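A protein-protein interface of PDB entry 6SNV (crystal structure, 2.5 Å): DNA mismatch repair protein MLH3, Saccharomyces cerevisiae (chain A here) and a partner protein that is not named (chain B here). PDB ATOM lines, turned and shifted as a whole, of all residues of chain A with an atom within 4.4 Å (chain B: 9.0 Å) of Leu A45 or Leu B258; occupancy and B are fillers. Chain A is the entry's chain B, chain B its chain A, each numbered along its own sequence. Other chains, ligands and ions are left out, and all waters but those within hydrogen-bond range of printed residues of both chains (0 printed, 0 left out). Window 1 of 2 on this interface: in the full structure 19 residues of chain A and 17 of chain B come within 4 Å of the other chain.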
ATOM      1  N   VAL A  23      -3.409  21.056 -13.590  1.00  0.00           N
ATOM      2  CA  VAL A  23      -3.905  19.724 -13.236  1.00  0.00           C
ATOM      3  C   VAL A  23      -5.190  19.439 -14.034  1.00  0.00           C
ATOM      4  O   VAL A  23      -6.133  20.227 -13.956  1.00  0.00           O
ATOM      5  CB  VAL A  23      -4.141  19.586 -11.700  1.00  0.00           C
ATOM      6  CG1 VAL A  23      -5.012  18.380 -11.365  1.00  0.00           C
ATOM      7  CG2 VAL A  23      -2.830  19.534 -10.931  1.00  0.00           C
ATOM      8  N   PHE A  27      -7.514  22.900 -13.270  1.00  0.00           N
ATOM      9  CA  PHE A  27      -6.980  23.573 -12.087  1.00  0.00           C
ATOM     10  C   PHE A  27      -5.552  24.017 -12.262  1.00  0.00           C
ATOM     11  O   PHE A  27      -4.892  23.655 -13.235  1.00  0.00           O
ATOM     12  CB  PHE A  27      -7.026  22.626 -10.870  1.00  0.00           C
ATOM     13  CG  PHE A  27      -8.353  21.966 -10.595  1.00  0.00           C
ATOM     14  CD1 PHE A  27      -9.312  22.598  -9.812  1.00  0.00           C
ATOM     15  CD2 PHE A  27      -8.649  20.716 -11.128  1.00  0.00           C
ATOM     16  CE1 PHE A  27     -10.542  21.988  -9.563  1.00  0.00           C
ATOM     17  CE2 PHE A  27      -9.890  20.119 -10.902  1.00  0.00           C
ATOM     18  CZ  PHE A  27     -10.821  20.750 -10.105  1.00  0.00           C
ATOM     19  N   ILE A  28      -5.064  24.775 -11.278  1.00  0.00           N
ATOM     20  CA  ILE A  28      -3.681  25.217 -11.156  1.00  0.00           C
ATOM     21  C   ILE A  28      -3.295  24.853  -9.735  1.00  0.00           C
ATOM     22  O   ILE A  28      -3.813  25.452  -8.778  1.00  0.00           O
ATOM     23  CB  ILE A  28      -3.447  26.726 -11.452  1.00  0.00           C
ATOM     24  CG1 ILE A  28      -3.859  27.105 -12.897  1.00  0.00           C
ATOM     25  CG2 ILE A  28      -1.984  27.106 -11.163  1.00  0.00           C
ATOM     26  CD1 ILE A  28      -4.376  28.521 -13.039  1.00  0.00           C
ATOM     27  N   LEU A  29      -2.427  23.837  -9.596  1.00  0.00           N
ATOM     28  CA  LEU A  29      -1.952  23.396  -8.290  1.00  0.00           C
ATOM     29  C   LEU A  29      -0.854  24.348  -7.846  1.00  0.00           C
ATOM     30  O   LEU A  29       0.090  24.593  -8.600  1.00  0.00           O
ATOM     31  CB  LEU A  29      -1.470  21.931  -8.332  1.00  0.00           C
ATOM     32  CG  LEU A  29      -0.931  21.331  -7.023  1.00  0.00           C
ATOM     33  CD1 LEU A  29      -2.042  21.081  -6.018  1.00  0.00           C
ATOM     34  CD2 LEU A  29      -0.165  20.056  -7.289  1.00  0.00           C
ATOM     35  N   VAL A  44      -2.913  24.052  -2.605  1.00  0.00           N
ATOM     36  CA  VAL A  44      -4.211  24.612  -2.960  1.00  0.00           C
ATOM     37  C   VAL A  44      -4.469  24.376  -4.456  1.00  0.00           C
ATOM     38  O   VAL A  44      -3.558  24.525  -5.273  1.00  0.00           O
ATOM     39  CB  VAL A  44      -4.319  26.115  -2.559  1.00  0.00           C
ATOM     40  CG1 VAL A  44      -5.688  26.694  -2.905  1.00  0.00           C
ATOM     41  CG2 VAL A  44      -4.024  26.326  -1.076  1.00  0.00           C
ATOM     42  N   LEU A  45      -5.706  23.961  -4.800  1.00  0.00           N
ATOM     43  CA  LEU A  45      -6.137  23.762  -6.179  1.00  0.00           C
ATOM     44  C   LEU A  45      -7.021  24.946  -6.560  1.00  0.00           C
ATOM     45  O   LEU A  45      -8.062  25.160  -5.944  1.00  0.00           O
ATOM     46  CB  LEU A  45      -6.899  22.434  -6.359  1.00  0.00           C
ATOM     47  CG  LEU A  45      -6.079  21.165  -6.630  1.00  0.00           C
ATOM     48  CD1 LEU A  45      -6.988  19.954  -6.688  1.00  0.00           C
ATOM     49  CD2 LEU A  45      -5.279  21.256  -7.938  1.00  0.00           C
ATOM     50  N   VAL A  46      -6.576  25.742  -7.541  1.00  0.00           N
ATOM     51  CA  VAL A  46      -7.281  26.934  -8.022  1.00  0.00           C
ATOM     52  C   VAL A  46      -8.023  26.614  -9.311  1.00  0.00           C
ATOM     53  O   VAL A  46      -7.402  26.160 -10.267  1.00  0.00           O
ATOM     54  CB  VAL A  46      -6.316  28.132  -8.224  1.00  0.00           C
ATOM     55  CG1 VAL A  46      -7.060  29.358  -8.740  1.00  0.00           C
ATOM     56  CG2 VAL A  46      -5.559  28.463  -6.945  1.00  0.00           C
ATOM     57  N   ASP A  47      -9.341  26.885  -9.346  1.00  0.00           N
ATOM     58  CA  ASP A  47     -10.188  26.719 -10.530  1.00  0.00           C
ATOM     59  C   ASP A  47      -9.719  27.778 -11.547  1.00  0.00           C
ATOM     60  O   ASP A  47      -9.796  28.979 -11.265  1.00  0.00           O
ATOM     61  CB  ASP A  47     -11.669  26.901 -10.141  1.00  0.00           C
ATOM     62  CG  ASP A  47     -12.692  26.974 -11.264  1.00  0.00           C
ATOM     63  OD1 ASP A  47     -12.302  26.841 -12.438  1.00  0.00           O
ATOM     64  OD2 ASP A  47     -13.881  27.191 -10.967  1.00  0.00           O
ATOM     65  N   MET A 232     -10.857  28.781  -5.345  1.00  0.00           N
ATOM     66  CA  MET A 232      -9.831  27.813  -4.960  1.00  0.00           C
ATOM     67  C   MET A 232     -10.247  26.915  -3.792  1.00  0.00           C
ATOM     68  O   MET A 232     -11.103  27.302  -2.992  1.00  0.00           O
ATOM     69  CB  MET A 232      -8.490  28.517  -4.681  1.00  0.00           C
ATOM     70  CG  MET A 232      -8.515  29.452  -3.502  1.00  0.00           C
ATOM     71  SD  MET A 232      -7.078  30.523  -3.472  1.00  0.00           S
ATOM     72  CE  MET A 232      -7.583  31.772  -4.618  1.00  0.00           C
ATOM     73  N   VAL A 233      -9.636  25.718  -3.702  1.00  0.00           N
ATOM     74  CA  VAL A 233      -9.881  24.725  -2.650  1.00  0.00           C
ATOM     75  C   VAL A 233      -8.541  24.161  -2.115  1.00  0.00           C
ATOM     76  O   VAL A 233      -7.744  23.656  -2.909  1.00  0.00           O
ATOM     77  CB  VAL A 233     -10.867  23.607  -3.120  1.00  0.00           C
ATOM     78  CG1 VAL A 233     -10.807  22.373  -2.224  1.00  0.00           C
ATOM     79  CG2 VAL A 233     -12.299  24.130  -3.191  1.00  0.00           C
ATOM     80  N   ILE A 235      -6.170  21.334  -0.641  1.00  0.00           N
ATOM     81  CA  ILE A 235      -6.207  19.865  -0.675  1.00  0.00           C
ATOM     82  C   ILE A 235      -5.333  19.200   0.411  1.00  0.00           C
ATOM     83  O   ILE A 235      -5.545  18.019   0.716  1.00  0.00           O
ATOM     84  CB  ILE A 235      -5.903  19.293  -2.087  1.00  0.00           C
ATOM     85  CG1 ILE A 235      -4.556  19.790  -2.655  1.00  0.00           C
ATOM     86  CG2 ILE A 235      -7.069  19.582  -3.037  1.00  0.00           C
ATOM     87  CD1 ILE A 235      -3.999  18.930  -3.742  1.00  0.00           C
ATOM     88  N   VAL B  35       2.767  15.938 -12.645  1.00  0.00           N
ATOM     89  CA  VAL B  35       2.280  17.311 -12.460  1.00  0.00           C
ATOM     90  C   VAL B  35       3.472  18.270 -12.222  1.00  0.00           C
ATOM     91  O   VAL B  35       3.685  19.181 -13.029  1.00  0.00           O
ATOM     92  CB  VAL B  35       1.169  17.407 -11.364  1.00  0.00           C
ATOM     93  CG1 VAL B  35       0.768  18.852 -11.084  1.00  0.00           C
ATOM     94  CG2 VAL B  35      -0.053  16.569 -11.732  1.00  0.00           C
ATOM     95  N   ALA B  46       4.195  15.644  -7.400  1.00  0.00           N
ATOM     96  CA  ALA B  46       2.778  15.330  -7.555  1.00  0.00           C
ATOM     97  C   ALA B  46       2.523  14.689  -8.898  1.00  0.00           C
ATOM     98  O   ALA B  46       3.124  15.082  -9.902  1.00  0.00           O
ATOM     99  CB  ALA B  46       1.927  16.574  -7.388  1.00  0.00           C
ATOM    100  N   GLN B  48      -0.772  12.382 -11.297  1.00  0.00           N
ATOM    101  CA  GLN B  48      -2.180  12.097 -11.463  1.00  0.00           C
ATOM    102  C   GLN B  48      -2.328  10.723 -12.069  1.00  0.00           C
ATOM    103  O   GLN B  48      -1.712  10.426 -13.090  1.00  0.00           O
ATOM    104  CB  GLN B  48      -2.873  13.157 -12.327  1.00  0.00           C
ATOM    105  CG  GLN B  48      -4.349  13.322 -11.989  1.00  0.00           C
ATOM    106  CD  GLN B  48      -5.121  13.979 -13.101  1.00  0.00           C
ATOM    107  OE1 GLN B  48      -4.818  15.111 -13.520  1.00  0.00           O
ATOM    108  NE2 GLN B  48      -6.150  13.284 -13.590  1.00  0.00           N
ATOM    109  N   LEU B  51      -8.207   9.827 -12.157  1.00  0.00           N
ATOM    110  CA  LEU B  51      -8.709  11.156 -11.795  1.00  0.00           C
ATOM    111  C   LEU B  51      -8.485  11.448 -10.303  1.00  0.00           C
ATOM    112  O   LEU B  51      -9.316  12.073  -9.644  1.00  0.00           O
ATOM    113  CB  LEU B  51     -10.179  11.350 -12.241  1.00  0.00           C
ATOM    114  CG  LEU B  51     -10.470  11.146 -13.745  1.00  0.00           C
ATOM    115  CD1 LEU B  51     -11.836  10.538 -13.969  1.00  0.00           C
ATOM    116  CD2 LEU B  51     -10.264  12.427 -14.550  1.00  0.00           C
ATOM    117  N   LYS B  52      -7.331  10.990  -9.784  1.00  0.00           N
ATOM    118  CA  LYS B  52      -6.890  11.161  -8.403  1.00  0.00           C
ATOM    119  C   LYS B  52      -5.503  11.776  -8.405  1.00  0.00           C
ATOM    120  O   LYS B  52      -4.650  11.388  -9.204  1.00  0.00           O
ATOM    121  CB  LYS B  52      -6.839   9.812  -7.672  1.00  0.00           C
ATOM    122  CG  LYS B  52      -8.181   9.285  -7.198  1.00  0.00           C
ATOM    123  CD  LYS B  52      -8.025   7.901  -6.589  1.00  0.00           C
ATOM    124  CE  LYS B  52      -9.327   7.355  -6.068  1.00  0.00           C
ATOM    125  NZ  LYS B  52      -9.121   6.094  -5.310  1.00  0.00           N
ATOM    126  N   LEU B  53      -5.274  12.724  -7.496  1.00  0.00           N
ATOM    127  CA  LEU B  53      -3.992  13.397  -7.334  1.00  0.00           C
ATOM    128  C   LEU B  53      -3.201  12.742  -6.198  1.00  0.00           C
ATOM    129  O   LEU B  53      -3.733  12.543  -5.102  1.00  0.00           O
ATOM    130  CB  LEU B  53      -4.201  14.897  -7.080  1.00  0.00           C
ATOM    131  CG  LEU B  53      -3.169  15.818  -7.720  1.00  0.00           C
ATOM    132  CD1 LEU B  53      -3.389  15.926  -9.219  1.00  0.00           C
ATOM    133  CD2 LEU B  53      -3.202  17.191  -7.086  1.00  0.00           C
ATOM    134  N   GLU B 251      -2.708   9.635  -1.579  1.00  0.00           N
ATOM    135  CA  GLU B 251      -3.739  10.325  -2.369  1.00  0.00           C
ATOM    136  C   GLU B 251      -4.079  11.640  -1.650  1.00  0.00           C
ATOM    137  O   GLU B 251      -4.540  11.610  -0.506  1.00  0.00           O
ATOM    138  CB  GLU B 251      -4.988   9.438  -2.556  1.00  0.00           C
ATOM    139  CG  GLU B 251      -6.065  10.041  -3.445  1.00  0.00           C
ATOM    140  CD  GLU B 251      -7.481   9.656  -3.062  1.00  0.00           C
ATOM    141  OE1 GLU B 251      -8.234  10.546  -2.604  1.00  0.00           O
ATOM    142  OE2 GLU B 251      -7.838   8.465  -3.214  1.00  0.00           O
ATOM    143  N   ILE B 252      -3.809  12.785  -2.299  1.00  0.00           N
ATOM    144  CA  ILE B 252      -4.048  14.110  -1.710  1.00  0.00           C
ATOM    145  C   ILE B 252      -5.414  14.696  -2.114  1.00  0.00           C
ATOM    146  O   ILE B 252      -5.947  15.546  -1.387  1.00  0.00           O
ATOM    147  CB  ILE B 252      -2.880  15.106  -1.951  1.00  0.00           C
ATOM    148  CG1 ILE B 252      -2.444  15.154  -3.439  1.00  0.00           C
ATOM    149  CG2 ILE B 252      -1.725  14.787  -1.002  1.00  0.00           C
ATOM    150  CD1 ILE B 252      -1.395  16.192  -3.802  1.00  0.00           C
ATOM    151  N   ALA B 253      -5.988  14.222  -3.247  1.00  0.00           N
ATOM    152  CA  ALA B 253      -7.300  14.656  -3.736  1.00  0.00           C
ATOM    153  C   ALA B 253      -7.928  13.678  -4.717  1.00  0.00           C
ATOM    154  O   ALA B 253      -7.234  13.101  -5.554  1.00  0.00           O
ATOM    155  CB  ALA B 253      -7.194  16.027  -4.390  1.00  0.00           C
ATOM    156  N   ASN B 254      -9.255  13.511  -4.613  1.00  0.00           N
ATOM    157  CA  ASN B 254     -10.076  12.730  -5.538  1.00  0.00           C
ATOM    158  C   ASN B 254     -10.793  13.822  -6.342  1.00  0.00           C
ATOM    159  O   ASN B 254     -11.669  14.507  -5.807  1.00  0.00           O
ATOM    160  CB  ASN B 254     -11.064  11.812  -4.790  1.00  0.00           C
ATOM    161  CG  ASN B 254     -11.897  10.934  -5.698  1.00  0.00           C
ATOM    162  OD1 ASN B 254     -11.399  10.005  -6.343  1.00  0.00           O
ATOM    163  ND2 ASN B 254     -13.193  11.206  -5.766  1.00  0.00           N
ATOM    164  N   LEU B 255     -10.338  14.051  -7.590  1.00  0.00           N
ATOM    165  CA  LEU B 255     -10.815  15.124  -8.470  1.00  0.00           C
ATOM    166  C   LEU B 255     -12.340  15.113  -8.747  1.00  0.00           C
ATOM    167  O   LEU B 255     -12.901  16.211  -8.713  1.00  0.00           O
ATOM    168  CB  LEU B 255     -10.012  15.197  -9.771  1.00  0.00           C
ATOM    169  CG  LEU B 255      -8.500  15.427  -9.593  1.00  0.00           C
ATOM    170  CD1 LEU B 255      -7.753  15.133 -10.868  1.00  0.00           C
ATOM    171  CD2 LEU B 255      -8.189  16.836  -9.066  1.00  0.00           C
ATOM    172  N   PRO B 256     -13.063  13.962  -8.914  1.00  0.00           N
ATOM    173  CA  PRO B 256     -14.529  14.036  -9.068  1.00  0.00           C
ATOM    174  C   PRO B 256     -15.239  14.858  -7.982  1.00  0.00           C
ATOM    175  O   PRO B 256     -16.186  15.581  -8.301  1.00  0.00           O
ATOM    176  CB  PRO B 256     -14.959  12.569  -9.031  1.00  0.00           C
ATOM    177  CG  PRO B 256     -13.787  11.832  -9.544  1.00  0.00           C
ATOM    178  CD  PRO B 256     -12.605  12.556  -8.982  1.00  0.00           C
ATOM    179  N   ASP B 257     -14.752  14.789  -6.719  1.00  0.00           N
ATOM    180  CA  ASP B 257     -15.284  15.549  -5.578  1.00  0.00           C
ATOM    181  C   ASP B 257     -15.105  17.056  -5.783  1.00  0.00           C
ATOM    182  O   ASP B 257     -15.980  17.829  -5.388  1.00  0.00           O
ATOM    183  CB  ASP B 257     -14.611  15.128  -4.259  1.00  0.00           C
ATOM    184  CG  ASP B 257     -14.580  13.638  -3.961  1.00  0.00           C
ATOM    185  OD1 ASP B 257     -15.418  12.897  -4.530  1.00  0.00           O
ATOM    186  OD2 ASP B 257     -13.726  13.215  -3.152  1.00  0.00           O
ATOM    187  N   LEU B 258     -13.972  17.471  -6.384  1.00  0.00           N
ATOM    188  CA  LEU B 258     -13.685  18.880  -6.658  1.00  0.00           C
ATOM    189  C   LEU B 258     -14.535  19.434  -7.796  1.00  0.00           C
ATOM    190  O   LEU B 258     -14.820  20.630  -7.786  1.00  0.00           O
ATOM    191  CB  LEU B 258     -12.198  19.104  -6.942  1.00  0.00           C
ATOM    192  CG  LEU B 258     -11.334  19.330  -5.711  1.00  0.00           C
ATOM    193  CD1 LEU B 258     -10.276  18.256  -5.592  1.00  0.00           C
ATOM    194  CD2 LEU B 258     -10.693  20.706  -5.739  1.00  0.00           C
ATOM    195  N   TYR B 259     -14.949  18.574  -8.768  1.00  0.00           N
ATOM    196  CA  TYR B 259     -15.784  18.969  -9.914  1.00  0.00           C
ATOM    197  C   TYR B 259     -17.125  19.551  -9.467  1.00  0.00           C
ATOM    198  O   TYR B 259     -17.630  20.452 -10.123  1.00  0.00           O
ATOM    199  CB  TYR B 259     -16.064  17.790 -10.870  1.00  0.00           C
ATOM    200  CG  TYR B 259     -14.872  17.121 -11.529  1.00  0.00           C
ATOM    201  CD1 TYR B 259     -13.686  17.815 -11.741  1.00  0.00           C
ATOM    202  CD2 TYR B 259     -14.974  15.829 -12.034  1.00  0.00           C
ATOM    203  CE1 TYR B 259     -12.595  17.204 -12.358  1.00  0.00           C
ATOM    204  CE2 TYR B 259     -13.891  15.209 -12.651  1.00  0.00           C
ATOM    205  CZ  TYR B 259     -12.707  15.903 -12.821  1.00  0.00           C
ATOM    206  OH  TYR B 259     -11.644  15.293 -13.436  1.00  0.00           O
ATOM    207  N   LYS B 260     -17.702  19.018  -8.368  1.00  0.00           N
ATOM    208  CA  LYS B 260     -18.970  19.441  -7.762  1.00  0.00           C
ATOM    209  C   LYS B 260     -18.890  20.892  -7.240  1.00  0.00           C
ATOM    210  O   LYS B 260     -19.863  21.636  -7.367  1.00  0.00           O
ATOM    211  CB  LYS B 260     -19.345  18.472  -6.620  1.00  0.00           C
ATOM    212  CG  LYS B 260     -20.785  18.582  -6.130  1.00  0.00           C
ATOM    213  CD  LYS B 260     -21.057  17.604  -4.997  1.00  0.00           C
ATOM    214  CE  LYS B 260     -22.476  17.695  -4.496  1.00  0.00           C
ATOM    215  NZ  LYS B 260     -22.752  16.686  -3.440  1.00  0.00           N
ATOM    216  N   VAL B 261     -17.728  21.278  -6.667  1.00  0.00           N
ATOM    217  CA  VAL B 261     -17.432  22.606  -6.099  1.00  0.00           C
ATOM    218  C   VAL B 261     -17.487  23.694  -7.181  1.00  0.00           C
ATOM    219  O   VAL B 261     -17.892  24.825  -6.896  1.00  0.00           O
ATOM    220  CB  VAL B 261     -16.059  22.628  -5.355  1.00  0.00           C
ATOM    221  CG1 VAL B 261     -15.894  23.894  -4.512  1.00  0.00           C
ATOM    222  CG2 VAL B 261     -15.855  21.377  -4.496  1.00  0.00           C
ATOM    223  N   PHE B 262     -17.076  23.348  -8.415  1.00  0.00           N
ATOM    224  CA  PHE B 262     -17.029  24.276  -9.545  1.00  0.00           C
ATOM    225  C   PHE B 262     -17.869  23.788 -10.739  1.00  0.00           C
ATOM    226  O   PHE B 262     -17.623  24.207 -11.872  1.00  0.00           O
ATOM    227  CB  PHE B 262     -15.562  24.535  -9.951  1.00  0.00           C
ATOM    228  CG  PHE B 262     -14.575  24.668  -8.809  1.00  0.00           C
ATOM    229  CD1 PHE B 262     -14.477  25.852  -8.087  1.00  0.00           C
ATOM    230  CD2 PHE B 262     -13.733  23.617  -8.470  1.00  0.00           C
ATOM    231  CE1 PHE B 262     -13.554  25.977  -7.045  1.00  0.00           C
ATOM    232  CE2 PHE B 262     -12.820  23.740  -7.422  1.00  0.00           C
ATOM    233  CZ  PHE B 262     -12.732  24.922  -6.721  1.00  0.00           C
ATOM    234  N   GLU B 263     -18.878  22.928 -10.469  1.00  0.00           N
ATOM    235  CA  GLU B 263     -19.797  22.342 -11.461  1.00  0.00           C
ATOM    236  C   GLU B 263     -20.584  23.431 -12.180  1.00  0.00           C
ATOM    237  O   GLU B 263     -20.635  23.444 -13.415  1.00  0.00           O
ATOM    238  CB  GLU B 263     -20.753  21.335 -10.787  1.00  0.00           C
ATOM    239  CG  GLU B 263     -21.452  20.406 -11.763  1.00  0.00           C
ATOM    240  CD  GLU B 263     -22.667  19.705 -11.190  1.00  0.00           C
ATOM    241  OE1 GLU B 263     -22.488  18.734 -10.421  1.00  0.00           O
ATOM    242  OE2 GLU B 263     -23.802  20.128 -11.513  1.00  0.00           O
ATOM    243  N   ARG B 264     -21.191  24.337 -11.396  1.00  0.00           N
ATOM    244  CA  ARG B 264     -21.963  25.478 -11.879  1.00  0.00           C
ATOM    245  C   ARG B 264     -21.203  26.731 -11.469  1.00  0.00           C
ATOM    246  O   ARG B 264     -20.948  26.938 -10.281  1.00  0.00           O
ATOM    247  CB  ARG B 264     -23.404  25.466 -11.317  1.00  0.00           C
ATOM    248  CG  ARG B 264     -24.256  24.323 -11.869  1.00  0.00           C
ATOM    249  CD  ARG B 264     -25.715  24.438 -11.483  1.00  0.00           C
ATOM    250  NE  ARG B 264     -26.508  23.363 -12.085  1.00  0.00           N
ATOM    251  CZ  ARG B 264     -27.837  23.319 -12.088  1.00  0.00           C
ATOM    252  NH1 ARG B 264     -28.470  22.302 -12.660  1.00  0.00           N
ATOM    253  NH2 ARG B 264     -28.544  24.290 -11.524  1.00  0.00           N
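Hydrophobic or aromatic side chains of chain A that line the printed part of chain B: Val A23, Phe A27, Leu A45, Val A233 and Ile A235.
Of the 20 printed residues of chain B, 8 touch a printed residue of chain A.
Printed residues of chain B that touch a printed residue of chain A: Val B35, Gln B48, Leu B53, Ile B252, Ala B253, Leu B258, Val B261 and Phe B262.
Hydrophobic or aromatic side chains of chain B within 4 Å of the printed part of chain A: Val B35, Leu B53, Ile B252, Ala B253, Leu B258, Val B261 and Phe B262.
Among the printed residues, 13 pairs touch across the chains.
Among the printed residues, no Asp or Glu carboxylate lies within 4 Å of a Lys or Arg side-chain nitrogen of the other chain.
The backbone carbonyl oxygen of Ala B46 lies within hydrogen-bond range of the backbone NH of Val B35.
O of Leu B53 lies within hydrogen-bond range of N of Ile B252, 2.8 Å away.
The backbone carbonyl oxygen of Ala B253 sits at hydrogen-bond distance from the backbone NH of Leu B53 (2.8 Å).
N of Val A233 is in hydrogen-bond range of O of Leu A45 (2.8 Å).
Among the printed residues, merely in contact across the chains: Asp A47 with Phe B262 (3.2 Å), Phe A27 with Phe B262 (3.6 Å), Val A23 with Leu B53 (3.6 Å), Val A233 with Phe B262 (3.6 Å), Val A23 with Val B35 (3.7 Å), Ile A235 with Ala B253 (3.8 Å), Phe A27 with Leu B258 (3.8 Å), Val A233 with Val B261 (3.8 Å), Ile A235 with Leu B53 (3.9 Å), Leu A45 with Leu B258 (3.9 Å), Val A233 with Leu B258 (3.9 Å) and Val A23 with Gln B48 (3.9 Å).
O of Ile A235 lies close to O of Ile B252, 3.3 Å away.
Of the printed residues of chain A, Leu B258 touches Phe A27 (3.8 Å), Leu A45 (3.9 Å) and Val A233 (3.9 Å).
Val A44 touches none of the printed residues of chain B.
Val A233 touches three residues of chain B.
Printed residues of chain A within 4 Å of Phe B262: Phe A27 (3.6 Å), Asp A47 (3.2 Å) and Val A233 (3.6 Å).
Printed residues of chain B within 4 Å of Phe A27: Leu B258 and Phe B262.
Of the printed residues of chain B, Asp A47 touches Phe B262.
Leu B255 touches none of the printed residues of chain A.
Lys B260 touches none of the printed residues of chain A.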
